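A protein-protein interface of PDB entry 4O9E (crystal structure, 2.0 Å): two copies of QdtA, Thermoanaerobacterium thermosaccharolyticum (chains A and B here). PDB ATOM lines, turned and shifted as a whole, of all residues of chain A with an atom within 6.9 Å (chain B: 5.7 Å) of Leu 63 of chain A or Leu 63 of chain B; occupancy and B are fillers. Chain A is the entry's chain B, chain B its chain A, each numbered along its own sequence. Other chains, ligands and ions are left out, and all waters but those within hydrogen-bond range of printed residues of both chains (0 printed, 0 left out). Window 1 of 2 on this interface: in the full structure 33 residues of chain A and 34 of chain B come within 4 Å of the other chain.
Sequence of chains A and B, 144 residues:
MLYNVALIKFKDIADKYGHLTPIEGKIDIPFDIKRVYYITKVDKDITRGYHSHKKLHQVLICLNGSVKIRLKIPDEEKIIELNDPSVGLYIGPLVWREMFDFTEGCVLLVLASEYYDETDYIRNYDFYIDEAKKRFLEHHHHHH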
ATOM      1  N   TYR A  37     -10.014  19.543   5.295  1.00  0.00           N
ATOM      2  CA  TYR A  37     -11.186  19.605   4.418  1.00  0.00           C
ATOM      3  C   TYR A  37     -11.523  21.049   4.106  1.00  0.00           C
ATOM      4  O   TYR A  37     -11.038  22.001   4.737  1.00  0.00           O
ATOM      5  CB  TYR A  37     -12.396  18.759   4.890  1.00  0.00           C
ATOM      6  CG  TYR A  37     -13.054  19.246   6.161  1.00  0.00           C
ATOM      7  CD1 TYR A  37     -14.081  20.198   6.120  1.00  0.00           C
ATOM      8  CD2 TYR A  37     -12.671  18.753   7.397  1.00  0.00           C
ATOM      9  CE1 TYR A  37     -14.688  20.639   7.280  1.00  0.00           C
ATOM     10  CE2 TYR A  37     -13.245  19.229   8.570  1.00  0.00           C
ATOM     11  CZ  TYR A  37     -14.271  20.162   8.503  1.00  0.00           C
ATOM     12  OH  TYR A  37     -14.901  20.674   9.616  1.00  0.00           O
ATOM     13  N   TYR A  38     -12.309  21.158   3.041  1.00  0.00           N
ATOM     14  CA  TYR A  38     -12.690  22.473   2.577  1.00  0.00           C
ATOM     15  C   TYR A  38     -14.100  22.481   1.968  1.00  0.00           C
ATOM     16  O   TYR A  38     -14.621  21.519   1.402  1.00  0.00           O
ATOM     17  CB  TYR A  38     -11.645  23.070   1.644  1.00  0.00           C
ATOM     18  CG  TYR A  38     -11.144  22.090   0.611  1.00  0.00           C
ATOM     19  CD1 TYR A  38     -11.793  21.874  -0.605  1.00  0.00           C
ATOM     20  CD2 TYR A  38     -10.009  21.332   0.860  1.00  0.00           C
ATOM     21  CE1 TYR A  38     -11.328  20.918  -1.508  1.00  0.00           C
ATOM     22  CE2 TYR A  38      -9.516  20.423  -0.067  1.00  0.00           C
ATOM     23  CZ  TYR A  38     -10.166  20.204  -1.266  1.00  0.00           C
ATOM     24  OH  TYR A  38      -9.616  19.303  -2.169  1.00  0.00           O
ATOM     25  N   ILE A  39     -14.734  23.610   2.241  1.00  0.00           N
ATOM     26  CA  ILE A  39     -16.150  23.824   1.969  1.00  0.00           C
ATOM     27  C   ILE A  39     -16.175  24.943   0.936  1.00  0.00           C
ATOM     28  O   ILE A  39     -15.525  25.974   1.118  1.00  0.00           O
ATOM     29  CB  ILE A  39     -16.825  24.234   3.280  1.00  0.00           C
ATOM     30  CG1 ILE A  39     -16.997  23.015   4.181  1.00  0.00           C
ATOM     31  CG2 ILE A  39     -18.198  24.867   3.042  1.00  0.00           C
ATOM     32  CD1 ILE A  39     -17.447  23.442   5.571  1.00  0.00           C
ATOM     33  N   THR A  40     -16.872  24.725  -0.177  1.00  0.00           N
ATOM     34  CA  THR A  40     -16.972  25.710  -1.258  1.00  0.00           C
ATOM     35  C   THR A  40     -18.437  25.792  -1.731  1.00  0.00           C
ATOM     36  O   THR A  40     -19.263  24.956  -1.369  1.00  0.00           O
ATOM     37  CB  THR A  40     -16.138  25.293  -2.480  1.00  0.00           C
ATOM     38  OG1 THR A  40     -16.450  23.936  -2.764  1.00  0.00           O
ATOM     39  CG2 THR A  40     -14.654  25.422  -2.204  1.00  0.00           C
ATOM     40  N   LYS A  41     -18.747  26.859  -2.464  1.00  0.00           N
ATOM     41  CA  LYS A  41     -19.996  27.002  -3.216  1.00  0.00           C
ATOM     42  C   LYS A  41     -21.197  26.931  -2.295  1.00  0.00           C
ATOM     43  O   LYS A  41     -22.140  26.174  -2.500  1.00  0.00           O
ATOM     44  CB  LYS A  41     -20.085  25.938  -4.303  1.00  0.00           C
ATOM     45  CG  LYS A  41     -18.983  26.067  -5.340  1.00  0.00           C
ATOM     46  CD  LYS A  41     -19.122  24.897  -6.302  1.00  0.00           C
ATOM     47  CE  LYS A  41     -17.840  24.153  -6.655  1.00  0.00           C
ATOM     48  NZ  LYS A  41     -16.868  23.712  -5.612  1.00  0.00           N
ATOM     49  N   ILE A  61      -9.862  28.387   8.323  1.00  0.00           N
ATOM     50  CA  ILE A  61      -9.163  29.430   7.606  1.00  0.00           C
ATOM     51  C   ILE A  61      -9.972  29.824   6.360  1.00  0.00           C
ATOM     52  O   ILE A  61     -10.296  29.004   5.495  1.00  0.00           O
ATOM     53  CB  ILE A  61      -7.749  29.005   7.196  1.00  0.00           C
ATOM     54  CG1 ILE A  61      -6.915  28.427   8.356  1.00  0.00           C
ATOM     55  CG2 ILE A  61      -7.000  30.233   6.746  1.00  0.00           C
ATOM     56  CD1 ILE A  61      -6.003  27.327   7.876  1.00  0.00           C
ATOM     57  N   CYS A  62     -10.324  31.103   6.265  1.00  0.00           N
ATOM     58  CA  CYS A  62     -11.076  31.549   5.069  1.00  0.00           C
ATOM     59  C   CYS A  62     -10.076  32.040   4.037  1.00  0.00           C
ATOM     60  O   CYS A  62      -9.400  33.057   4.194  1.00  0.00           O
ATOM     61  CB  CYS A  62     -12.135  32.617   5.374  1.00  0.00           C
ATOM     62  SG  CYS A  62     -12.848  33.218   3.825  1.00  0.00           S
ATOM     63  N   LEU A  63      -9.915  31.255   2.978  1.00  0.00           N
ATOM     64  CA  LEU A  63      -8.893  31.496   1.951  1.00  0.00           C
ATOM     65  C   LEU A  63      -9.305  32.398   0.782  1.00  0.00           C
ATOM     66  O   LEU A  63      -8.440  32.814  -0.001  1.00  0.00           O
ATOM     67  CB  LEU A  63      -8.489  30.178   1.283  1.00  0.00           C
ATOM     68  CG  LEU A  63      -7.993  29.036   2.182  1.00  0.00           C
ATOM     69  CD1 LEU A  63      -7.338  27.935   1.367  1.00  0.00           C
ATOM     70  CD2 LEU A  63      -7.024  29.676   3.153  1.00  0.00           C
ATOM     71  N   ASN A  64     -10.601  32.647   0.671  1.00  0.00           N
ATOM     72  CA  ASN A  64     -11.151  33.605  -0.310  1.00  0.00           C
ATOM     73  C   ASN A  64     -12.472  34.110   0.245  1.00  0.00           C
ATOM     74  O   ASN A  64     -13.207  33.361   0.910  1.00  0.00           O
ATOM     75  CB  ASN A  64     -11.394  32.994  -1.681  1.00  0.00           C
ATOM     76  CG  ASN A  64     -11.636  34.066  -2.752  1.00  0.00           C
ATOM     77  OD1 ASN A  64     -10.901  35.044  -2.836  1.00  0.00           O
ATOM     78  ND2 ASN A  64     -12.661  33.872  -3.561  1.00  0.00           N
ATOM     79  N   GLY A  65     -12.810  35.371  -0.014  1.00  0.00           N
ATOM     80  CA  GLY A  65     -14.172  35.754   0.324  1.00  0.00           C
ATOM     81  C   GLY A  65     -14.256  35.929   1.832  1.00  0.00           C
ATOM     82  O   GLY A  65     -13.261  36.212   2.520  1.00  0.00           O
ATOM     83  N   LEU A  82     -14.322  35.550   9.247  1.00  0.00           N
ATOM     84  CA  LEU A  82     -12.992  35.228   8.748  1.00  0.00           C
ATOM     85  C   LEU A  82     -12.951  35.737   7.326  1.00  0.00           C
ATOM     86  O   LEU A  82     -13.852  35.429   6.569  1.00  0.00           O
ATOM     87  CB  LEU A  82     -12.755  33.727   8.731  1.00  0.00           C
ATOM     88  CG  LEU A  82     -12.802  33.053  10.102  1.00  0.00           C
ATOM     89  CD1 LEU A  82     -12.741  31.556   9.820  1.00  0.00           C
ATOM     90  CD2 LEU A  82     -11.698  33.522  11.047  1.00  0.00           C
ATOM     91  N   ASN A  83     -11.896  36.467   6.996  1.00  0.00           N
ATOM     92  CA  ASN A  83     -11.769  37.120   5.709  1.00  0.00           C
ATOM     93  C   ASN A  83     -10.321  37.413   5.368  1.00  0.00           C
ATOM     94  O   ASN A  83     -10.080  38.187   4.454  1.00  0.00           O
ATOM     95  CB  ASN A  83     -12.545  38.442   5.720  1.00  0.00           C
ATOM     96  CG  ASN A  83     -12.205  39.303   6.912  1.00  0.00           C
ATOM     97  OD1 ASN A  83     -11.084  39.307   7.405  1.00  0.00           O
ATOM     98  ND2 ASN A  83     -13.179  40.057   7.384  1.00  0.00           N
ATOM     99  N   ASP A  84      -9.373  36.807   6.081  1.00  0.00           N
ATOM    100  CA  ASP A  84      -7.948  36.962   5.817  1.00  0.00           C
ATOM    101  C   ASP A  84      -7.260  35.586   5.734  1.00  0.00           C
ATOM    102  O   ASP A  84      -7.375  34.789   6.676  1.00  0.00           O
ATOM    103  CB  ASP A  84      -7.399  37.792   6.985  1.00  0.00           C
ATOM    104  CG  ASP A  84      -5.953  38.195   6.816  1.00  0.00           C
ATOM    105  OD1 ASP A  84      -5.208  37.559   6.042  1.00  0.00           O
ATOM    106  OD2 ASP A  84      -5.541  39.167   7.484  1.00  0.00           O
ATOM    107  N   PRO A  85      -6.551  35.284   4.632  1.00  0.00           N
ATOM    108  CA  PRO A  85      -6.057  33.911   4.645  1.00  0.00           C
ATOM    109  C   PRO A  85      -4.894  33.644   5.586  1.00  0.00           C
ATOM    110  O   PRO A  85      -4.594  32.482   5.852  1.00  0.00           O
ATOM    111  CB  PRO A  85      -5.660  33.649   3.191  1.00  0.00           C
ATOM    112  CG  PRO A  85      -6.430  34.656   2.387  1.00  0.00           C
ATOM    113  CD  PRO A  85      -6.749  35.808   3.265  1.00  0.00           C
ATOM    114  N   SER A  86      -4.206  34.687   6.047  1.00  0.00           N
ATOM    115  CA  SER A  86      -3.138  34.516   7.009  1.00  0.00           C
ATOM    116  C   SER A  86      -3.657  34.332   8.440  1.00  0.00           C
ATOM    117  O   SER A  86      -2.854  34.343   9.370  1.00  0.00           O
ATOM    118  CB  SER A  86      -2.210  35.727   6.923  1.00  0.00           C
ATOM    119  OG  SER A  86      -2.872  36.875   7.442  1.00  0.00           O
ATOM    120  N   GLY A 105     -17.032  33.444  -4.286  1.00  0.00           N
ATOM    121  CA  GLY A 105     -16.702  32.055  -4.006  1.00  0.00           C
ATOM    122  C   GLY A 105     -15.732  31.987  -2.831  1.00  0.00           C
ATOM    123  O   GLY A 105     -14.503  31.918  -2.951  1.00  0.00           O
ATOM    124  N   CYS A 106     -16.361  32.039  -1.664  1.00  0.00           N
ATOM    125  CA  CYS A 106     -15.767  31.820  -0.354  1.00  0.00           C
ATOM    126  C   CYS A 106     -15.161  30.420  -0.289  1.00  0.00           C
ATOM    127  O   CYS A 106     -15.782  29.452  -0.748  1.00  0.00           O
ATOM    128  CB  CYS A 106     -16.844  31.804   0.719  1.00  0.00           C
ATOM    129  SG  CYS A 106     -16.196  31.580   2.407  1.00  0.00           S
ATOM    130  N   VAL A 107     -13.952  30.340   0.266  1.00  0.00           N
ATOM    131  CA  VAL A 107     -13.325  29.033   0.494  1.00  0.00           C
ATOM    132  C   VAL A 107     -12.966  28.889   1.964  1.00  0.00           C
ATOM    133  O   VAL A 107     -12.297  29.765   2.474  1.00  0.00           O
ATOM    134  CB  VAL A 107     -12.034  28.934  -0.323  1.00  0.00           C
ATOM    135  CG1 VAL A 107     -11.330  27.636   0.053  1.00  0.00           C
ATOM    136  CG2 VAL A 107     -12.356  29.009  -1.810  1.00  0.00           C
ATOM    137  N   LEU A 108     -13.447  27.868   2.657  1.00  0.00           N
ATOM    138  CA  LEU A 108     -13.207  27.709   4.083  1.00  0.00           C
ATOM    139  C   LEU A 108     -12.457  26.379   4.220  1.00  0.00           C
ATOM    140  O   LEU A 108     -12.959  25.349   3.782  1.00  0.00           O
ATOM    141  CB  LEU A 108     -14.518  27.592   4.852  1.00  0.00           C
ATOM    142  CG  LEU A 108     -14.354  27.305   6.343  1.00  0.00           C
ATOM    143  CD1 LEU A 108     -13.596  28.422   7.039  1.00  0.00           C
ATOM    144  CD2 LEU A 108     -15.688  27.044   7.013  1.00  0.00           C
ATOM    145  N   LEU A 109     -11.217  26.444   4.696  1.00  0.00           N
ATOM    146  CA  LEU A 109     -10.340  25.290   4.831  1.00  0.00           C
ATOM    147  C   LEU A 109     -10.290  24.998   6.322  1.00  0.00           C
ATOM    148  O   LEU A 109     -10.280  25.912   7.144  1.00  0.00           O
ATOM    149  CB  LEU A 109      -8.949  25.648   4.327  1.00  0.00           C
ATOM    150  CG  LEU A 109      -7.829  24.662   4.663  1.00  0.00           C
ATOM    151  CD1 LEU A 109      -7.887  23.419   3.795  1.00  0.00           C
ATOM    152  CD2 LEU A 109      -6.535  25.411   4.415  1.00  0.00           C
ATOM    153  N   TYR B  38      -0.768  27.679   0.851  1.00  0.00           N
ATOM    154  CA  TYR B  38      -1.728  28.149  -0.118  1.00  0.00           C
ATOM    155  C   TYR B  38      -1.303  29.483  -0.719  1.00  0.00           C
ATOM    156  O   TYR B  38      -0.742  30.389  -0.087  1.00  0.00           O
ATOM    157  CB  TYR B  38      -3.159  28.213   0.405  1.00  0.00           C
ATOM    158  CG  TYR B  38      -3.303  28.673   1.829  1.00  0.00           C
ATOM    159  CD1 TYR B  38      -3.347  30.032   2.131  1.00  0.00           C
ATOM    160  CD2 TYR B  38      -3.481  27.765   2.859  1.00  0.00           C
ATOM    161  CE1 TYR B  38      -3.470  30.474   3.430  1.00  0.00           C
ATOM    162  CE2 TYR B  38      -3.591  28.204   4.168  1.00  0.00           C
ATOM    163  CZ  TYR B  38      -3.599  29.565   4.454  1.00  0.00           C
ATOM    164  OH  TYR B  38      -3.727  30.021   5.755  1.00  0.00           O
ATOM    165  N   THR B  40      -2.582  32.761  -3.125  1.00  0.00           N
ATOM    166  CA  THR B  40      -3.737  33.583  -3.422  1.00  0.00           C
ATOM    167  C   THR B  40      -3.298  34.939  -4.005  1.00  0.00           C
ATOM    168  O   THR B  40      -2.123  35.291  -3.978  1.00  0.00           O
ATOM    169  CB  THR B  40      -4.548  33.867  -2.139  1.00  0.00           C
ATOM    170  OG1 THR B  40      -3.732  34.558  -1.186  1.00  0.00           O
ATOM    171  CG2 THR B  40      -5.142  32.615  -1.539  1.00  0.00           C
ATOM    172  N   LYS B  41      -4.256  35.704  -4.521  1.00  0.00           N
ATOM    173  CA  LYS B  41      -4.032  37.100  -4.949  1.00  0.00           C
ATOM    174  C   LYS B  41      -2.882  37.243  -5.937  1.00  0.00           C
ATOM    175  O   LYS B  41      -2.072  38.170  -5.850  1.00  0.00           O
ATOM    176  CB  LYS B  41      -3.796  38.030  -3.738  1.00  0.00           C
ATOM    177  CG  LYS B  41      -4.962  38.046  -2.759  1.00  0.00           C
ATOM    178  CD  LYS B  41      -4.772  38.892  -1.507  1.00  0.00           C
ATOM    179  CE  LYS B  41      -4.049  38.177  -0.367  1.00  0.00           C
ATOM    180  NZ  LYS B  41      -4.819  37.020   0.180  1.00  0.00           N
ATOM    181  N   ILE B  61      -4.087  21.485  -5.493  1.00  0.00           N
ATOM    182  CA  ILE B  61      -5.535  21.535  -5.585  1.00  0.00           C
ATOM    183  C   ILE B  61      -5.986  22.987  -5.784  1.00  0.00           C
ATOM    184  O   ILE B  61      -5.604  23.882  -5.023  1.00  0.00           O
ATOM    185  CB  ILE B  61      -6.230  21.013  -4.314  1.00  0.00           C
ATOM    186  CG1 ILE B  61      -5.546  19.727  -3.864  1.00  0.00           C
ATOM    187  CG2 ILE B  61      -7.695  20.714  -4.557  1.00  0.00           C
ATOM    188  CD1 ILE B  61      -6.033  19.299  -2.507  1.00  0.00           C
ATOM    189  N   CYS B  62      -6.771  23.234  -6.832  1.00  0.00           N
ATOM    190  CA  CYS B  62      -7.316  24.584  -6.995  1.00  0.00           C
ATOM    191  C   CYS B  62      -8.724  24.635  -6.380  1.00  0.00           C
ATOM    192  O   CYS B  62      -9.687  24.003  -6.827  1.00  0.00           O
ATOM    193  CB  CYS B  62      -7.232  25.015  -8.472  1.00  0.00           C
ATOM    194  SG  CYS B  62      -8.042  26.610  -8.713  1.00  0.00           S
ATOM    195  N   LEU B  63      -8.837  25.344  -5.264  1.00  0.00           N
ATOM    196  CA  LEU B  63     -10.091  25.374  -4.541  1.00  0.00           C
ATOM    197  C   LEU B  63     -11.119  26.404  -5.044  1.00  0.00           C
ATOM    198  O   LEU B  63     -12.263  26.379  -4.599  1.00  0.00           O
ATOM    199  CB  LEU B  63      -9.810  25.656  -3.070  1.00  0.00           C
ATOM    200  CG  LEU B  63      -8.732  24.866  -2.313  1.00  0.00           C
ATOM    201  CD1 LEU B  63      -8.862  25.085  -0.808  1.00  0.00           C
ATOM    202  CD2 LEU B  63      -8.938  23.425  -2.726  1.00  0.00           C
ATOM    203  N   ASN B  64     -10.696  27.339  -5.881  1.00  0.00           N
ATOM    204  CA  ASN B  64     -11.575  28.377  -6.445  1.00  0.00           C
ATOM    205  C   ASN B  64     -10.885  28.881  -7.705  1.00  0.00           C
ATOM    206  O   ASN B  64      -9.672  29.109  -7.697  1.00  0.00           O
ATOM    207  CB  ASN B  64     -11.772  29.573  -5.507  1.00  0.00           C
ATOM    208  CG  ASN B  64     -12.778  30.589  -6.052  1.00  0.00           C
ATOM    209  OD1 ASN B  64     -13.927  30.252  -6.315  1.00  0.00           O
ATOM    210  ND2 ASN B  64     -12.379  31.845  -6.129  1.00  0.00           N
ATOM    211  N   GLY B  65     -11.658  29.104  -8.765  1.00  0.00           N
ATOM    212  CA  GLY B  65     -11.103  29.671  -9.988  1.00  0.00           C
ATOM    213  C   GLY B  65     -10.333  28.618 -10.759  1.00  0.00           C
ATOM    214  O   GLY B  65     -10.674  27.448 -10.744  1.00  0.00           O
ATOM    215  N   PRO B  85     -12.159  21.749  -7.271  1.00  0.00           N
ATOM    216  CA  PRO B  85     -11.609  21.479  -5.934  1.00  0.00           C
ATOM    217  C   PRO B  85     -11.534  20.022  -5.456  1.00  0.00           C
ATOM    218  O   PRO B  85     -11.001  19.746  -4.373  1.00  0.00           O
ATOM    219  CB  PRO B  85     -12.561  22.245  -5.010  1.00  0.00           C
ATOM    220  CG  PRO B  85     -13.235  23.295  -5.856  1.00  0.00           C
ATOM    221  CD  PRO B  85     -13.319  22.664  -7.225  1.00  0.00           C
ATOM    222  N   VAL B 107      -7.494  30.189  -5.707  1.00  0.00           N
ATOM    223  CA  VAL B 107      -6.836  29.699  -4.488  1.00  0.00           C
ATOM    224  C   VAL B 107      -6.212  28.344  -4.816  1.00  0.00           C
ATOM    225  O   VAL B 107      -6.877  27.438  -5.313  1.00  0.00           O
ATOM    226  CB  VAL B 107      -7.874  29.440  -3.377  1.00  0.00           C
ATOM    227  CG1 VAL B 107      -7.210  28.812  -2.159  1.00  0.00           C
ATOM    228  CG2 VAL B 107      -8.597  30.714  -2.970  1.00  0.00           C
ATOM    229  N   LEU B 108      -4.901  28.253  -4.626  1.00  0.00           N
ATOM    230  CA  LEU B 108      -4.153  27.045  -4.918  1.00  0.00           C
ATOM    231  C   LEU B 108      -3.550  26.576  -3.594  1.00  0.00           C
ATOM    232  O   LEU B 108      -2.749  27.285  -2.991  1.00  0.00           O
ATOM    233  CB  LEU B 108      -2.996  27.325  -5.866  1.00  0.00           C
ATOM    234  CG  LEU B 108      -2.130  26.148  -6.306  1.00  0.00           C
ATOM    235  CD1 LEU B 108      -2.853  25.057  -7.058  1.00  0.00           C
ATOM    236  CD2 LEU B 108      -0.864  26.494  -7.070  1.00  0.00           C
ATOM    237  N   LEU B 109      -3.990  25.385  -3.221  1.00  0.00           N
ATOM    238  CA  LEU B 109      -3.594  24.695  -1.995  1.00  0.00           C
ATOM    239  C   LEU B 109      -2.601  23.609  -2.374  1.00  0.00           C
ATOM    240  O   LEU B 109      -2.744  22.948  -3.403  1.00  0.00           O
ATOM    241  CB  LEU B 109      -4.816  24.089  -1.326  1.00  0.00           C
ATOM    242  CG  LEU B 109      -4.551  23.172  -0.126  1.00  0.00           C
ATOM    243  CD1 LEU B 109      -4.141  23.986   1.083  1.00  0.00           C
ATOM    244  CD2 LEU B 109      -5.867  22.482   0.144  1.00  0.00           C
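Tyr 38 of chain A touches Leu 63 of chain B, and with the chains exchanged Leu 63 of chain A touches Tyr 38 of chain B. Thr 40 of chain A touches Leu 63 of chain B, and with the chains exchanged Leu 63 of chain A touches Thr 40 of chain B. Leu 63 of chain A touches Val 107 of chain B, and with the chains exchanged Val 107 of chain A touches Leu 63 of chain B. Asn 64 of chain A touches its own counterpart, Asn 64 of chain B. Positions printed for both chains: 38, 40, 41, 61, 62, 63, 64, 65, 85, 107, 108 and 109. Of the 17 pairs that touch across the chains among the printed residues, 16 have their exchanged pair printed and touching as well.
The backbone carbonyl oxygen (O) of Asn 64 of chain A lies close to the side-chain sulfur (SG) of Cys 106 of chain A, 3.8 Å away. The backbone NH (N) of Val 107 of chain A sits at hydrogen-bond distance from the backbone carbonyl oxygen (O) of Asn 64 of chain A. The backbone carbonyl oxygen (O) of Ile 61 of chain B sits at hydrogen-bond distance from the backbone NH (N) of Leu 109 of chain B (2.8 Å). The backbone NH (N) of Ile 61 of chain A lies within hydrogen-bond range of the backbone carbonyl oxygen (O) of Leu 109 of chain A, at 2.8 Å. NZ of Lys 41 of chain B sits at hydrogen-bond distance from OG1 of Thr 40 of chain B (3.0 Å). The side-chain sulfur (SG) of Cys 62 of chain A sits close to the backbone carbonyl oxygen (O) of Val 107 of chain A (3.7 Å).
The side-chain amide nitrogen (ND2) of Asn 64 of chain B sits close to the side-chain amide nitrogen (ND2) of Asn 64 of chain A (3.3 Å). The backbone carbonyl oxygen (O) of Pro 85 of chain A lies within hydrogen-bond range of the side-chain hydroxyl (OH) of Tyr 38 of chain B, at 2.6 Å. O of Pro 85 of chain B lies within hydrogen-bond range of OH of Tyr 38 of chain A.
CE1 of Tyr 38 of chain A touches CD2 of Leu 63 of chain B (3.7 Å). Lys 41 of chain A touches Pro 85 of chain B. Tyr 38 of chain B touches Ile 61 of chain A. CE1 of Tyr 38 of chain B touches CD2 of Leu 63 of chain A (3.7 Å). Thr 40 of chain B touches Leu 63 of chain A. Leu 63 of chain A touches Leu 63 of chain B. Leu 63 of chain A touches Val 107 of chain B (CD1 to CG1, 3.6 Å). Lys 41 of chain B touches Pro 85 of chain A. Val 107 of chain A touches Leu 63 of chain B (CG1 to CD1, 3.7 Å). CB of Asn 64 of chain B touches CG2 of Val 107 of chain A, at 3.8 Å.
Leu 63 of chain A touches four residues of chain B. Printed residues of chain A within 4 Å of Ile 61 of chain B: Tyr 38. Printed residues of chain A within 4 Å of Lys 41 of chain B: Pro 85. Ser 86 of chain A touches none of the printed residues of chain B. The nearest residue of chain B that does not touch Leu 63 of chain A is Leu 109 of chain B (5.1 Å). The nearest printed residue of chain A that does not touch Thr 40 of chain B is Pro 85 of chain A (4.5 Å).
Of the 20 printed residues of chain A, 9 touch a printed residue of chain B. Hydrophobic or aromatic side chains of chain A within 4 Å of the printed part of chain B: Tyr 38, Ile 61, Leu 63, Pro 85 and Val 107. Of the 12 printed residues of chain B, 8 touch a printed residue of chain A. Printed residues of chain B that touch a printed residue of chain A: Tyr 38, Thr 40, Lys 41, Ile 61, Leu 63, Asn 64, Pro 85 and Val 107. Hydrophobic or aromatic side chains of chain B that line the printed part of chain A: Tyr 38, Ile 61, Leu 63, Pro 85 and Val 107. Along chain B the printed residues that touch a printed residue of chain A span positions 38 to 107.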
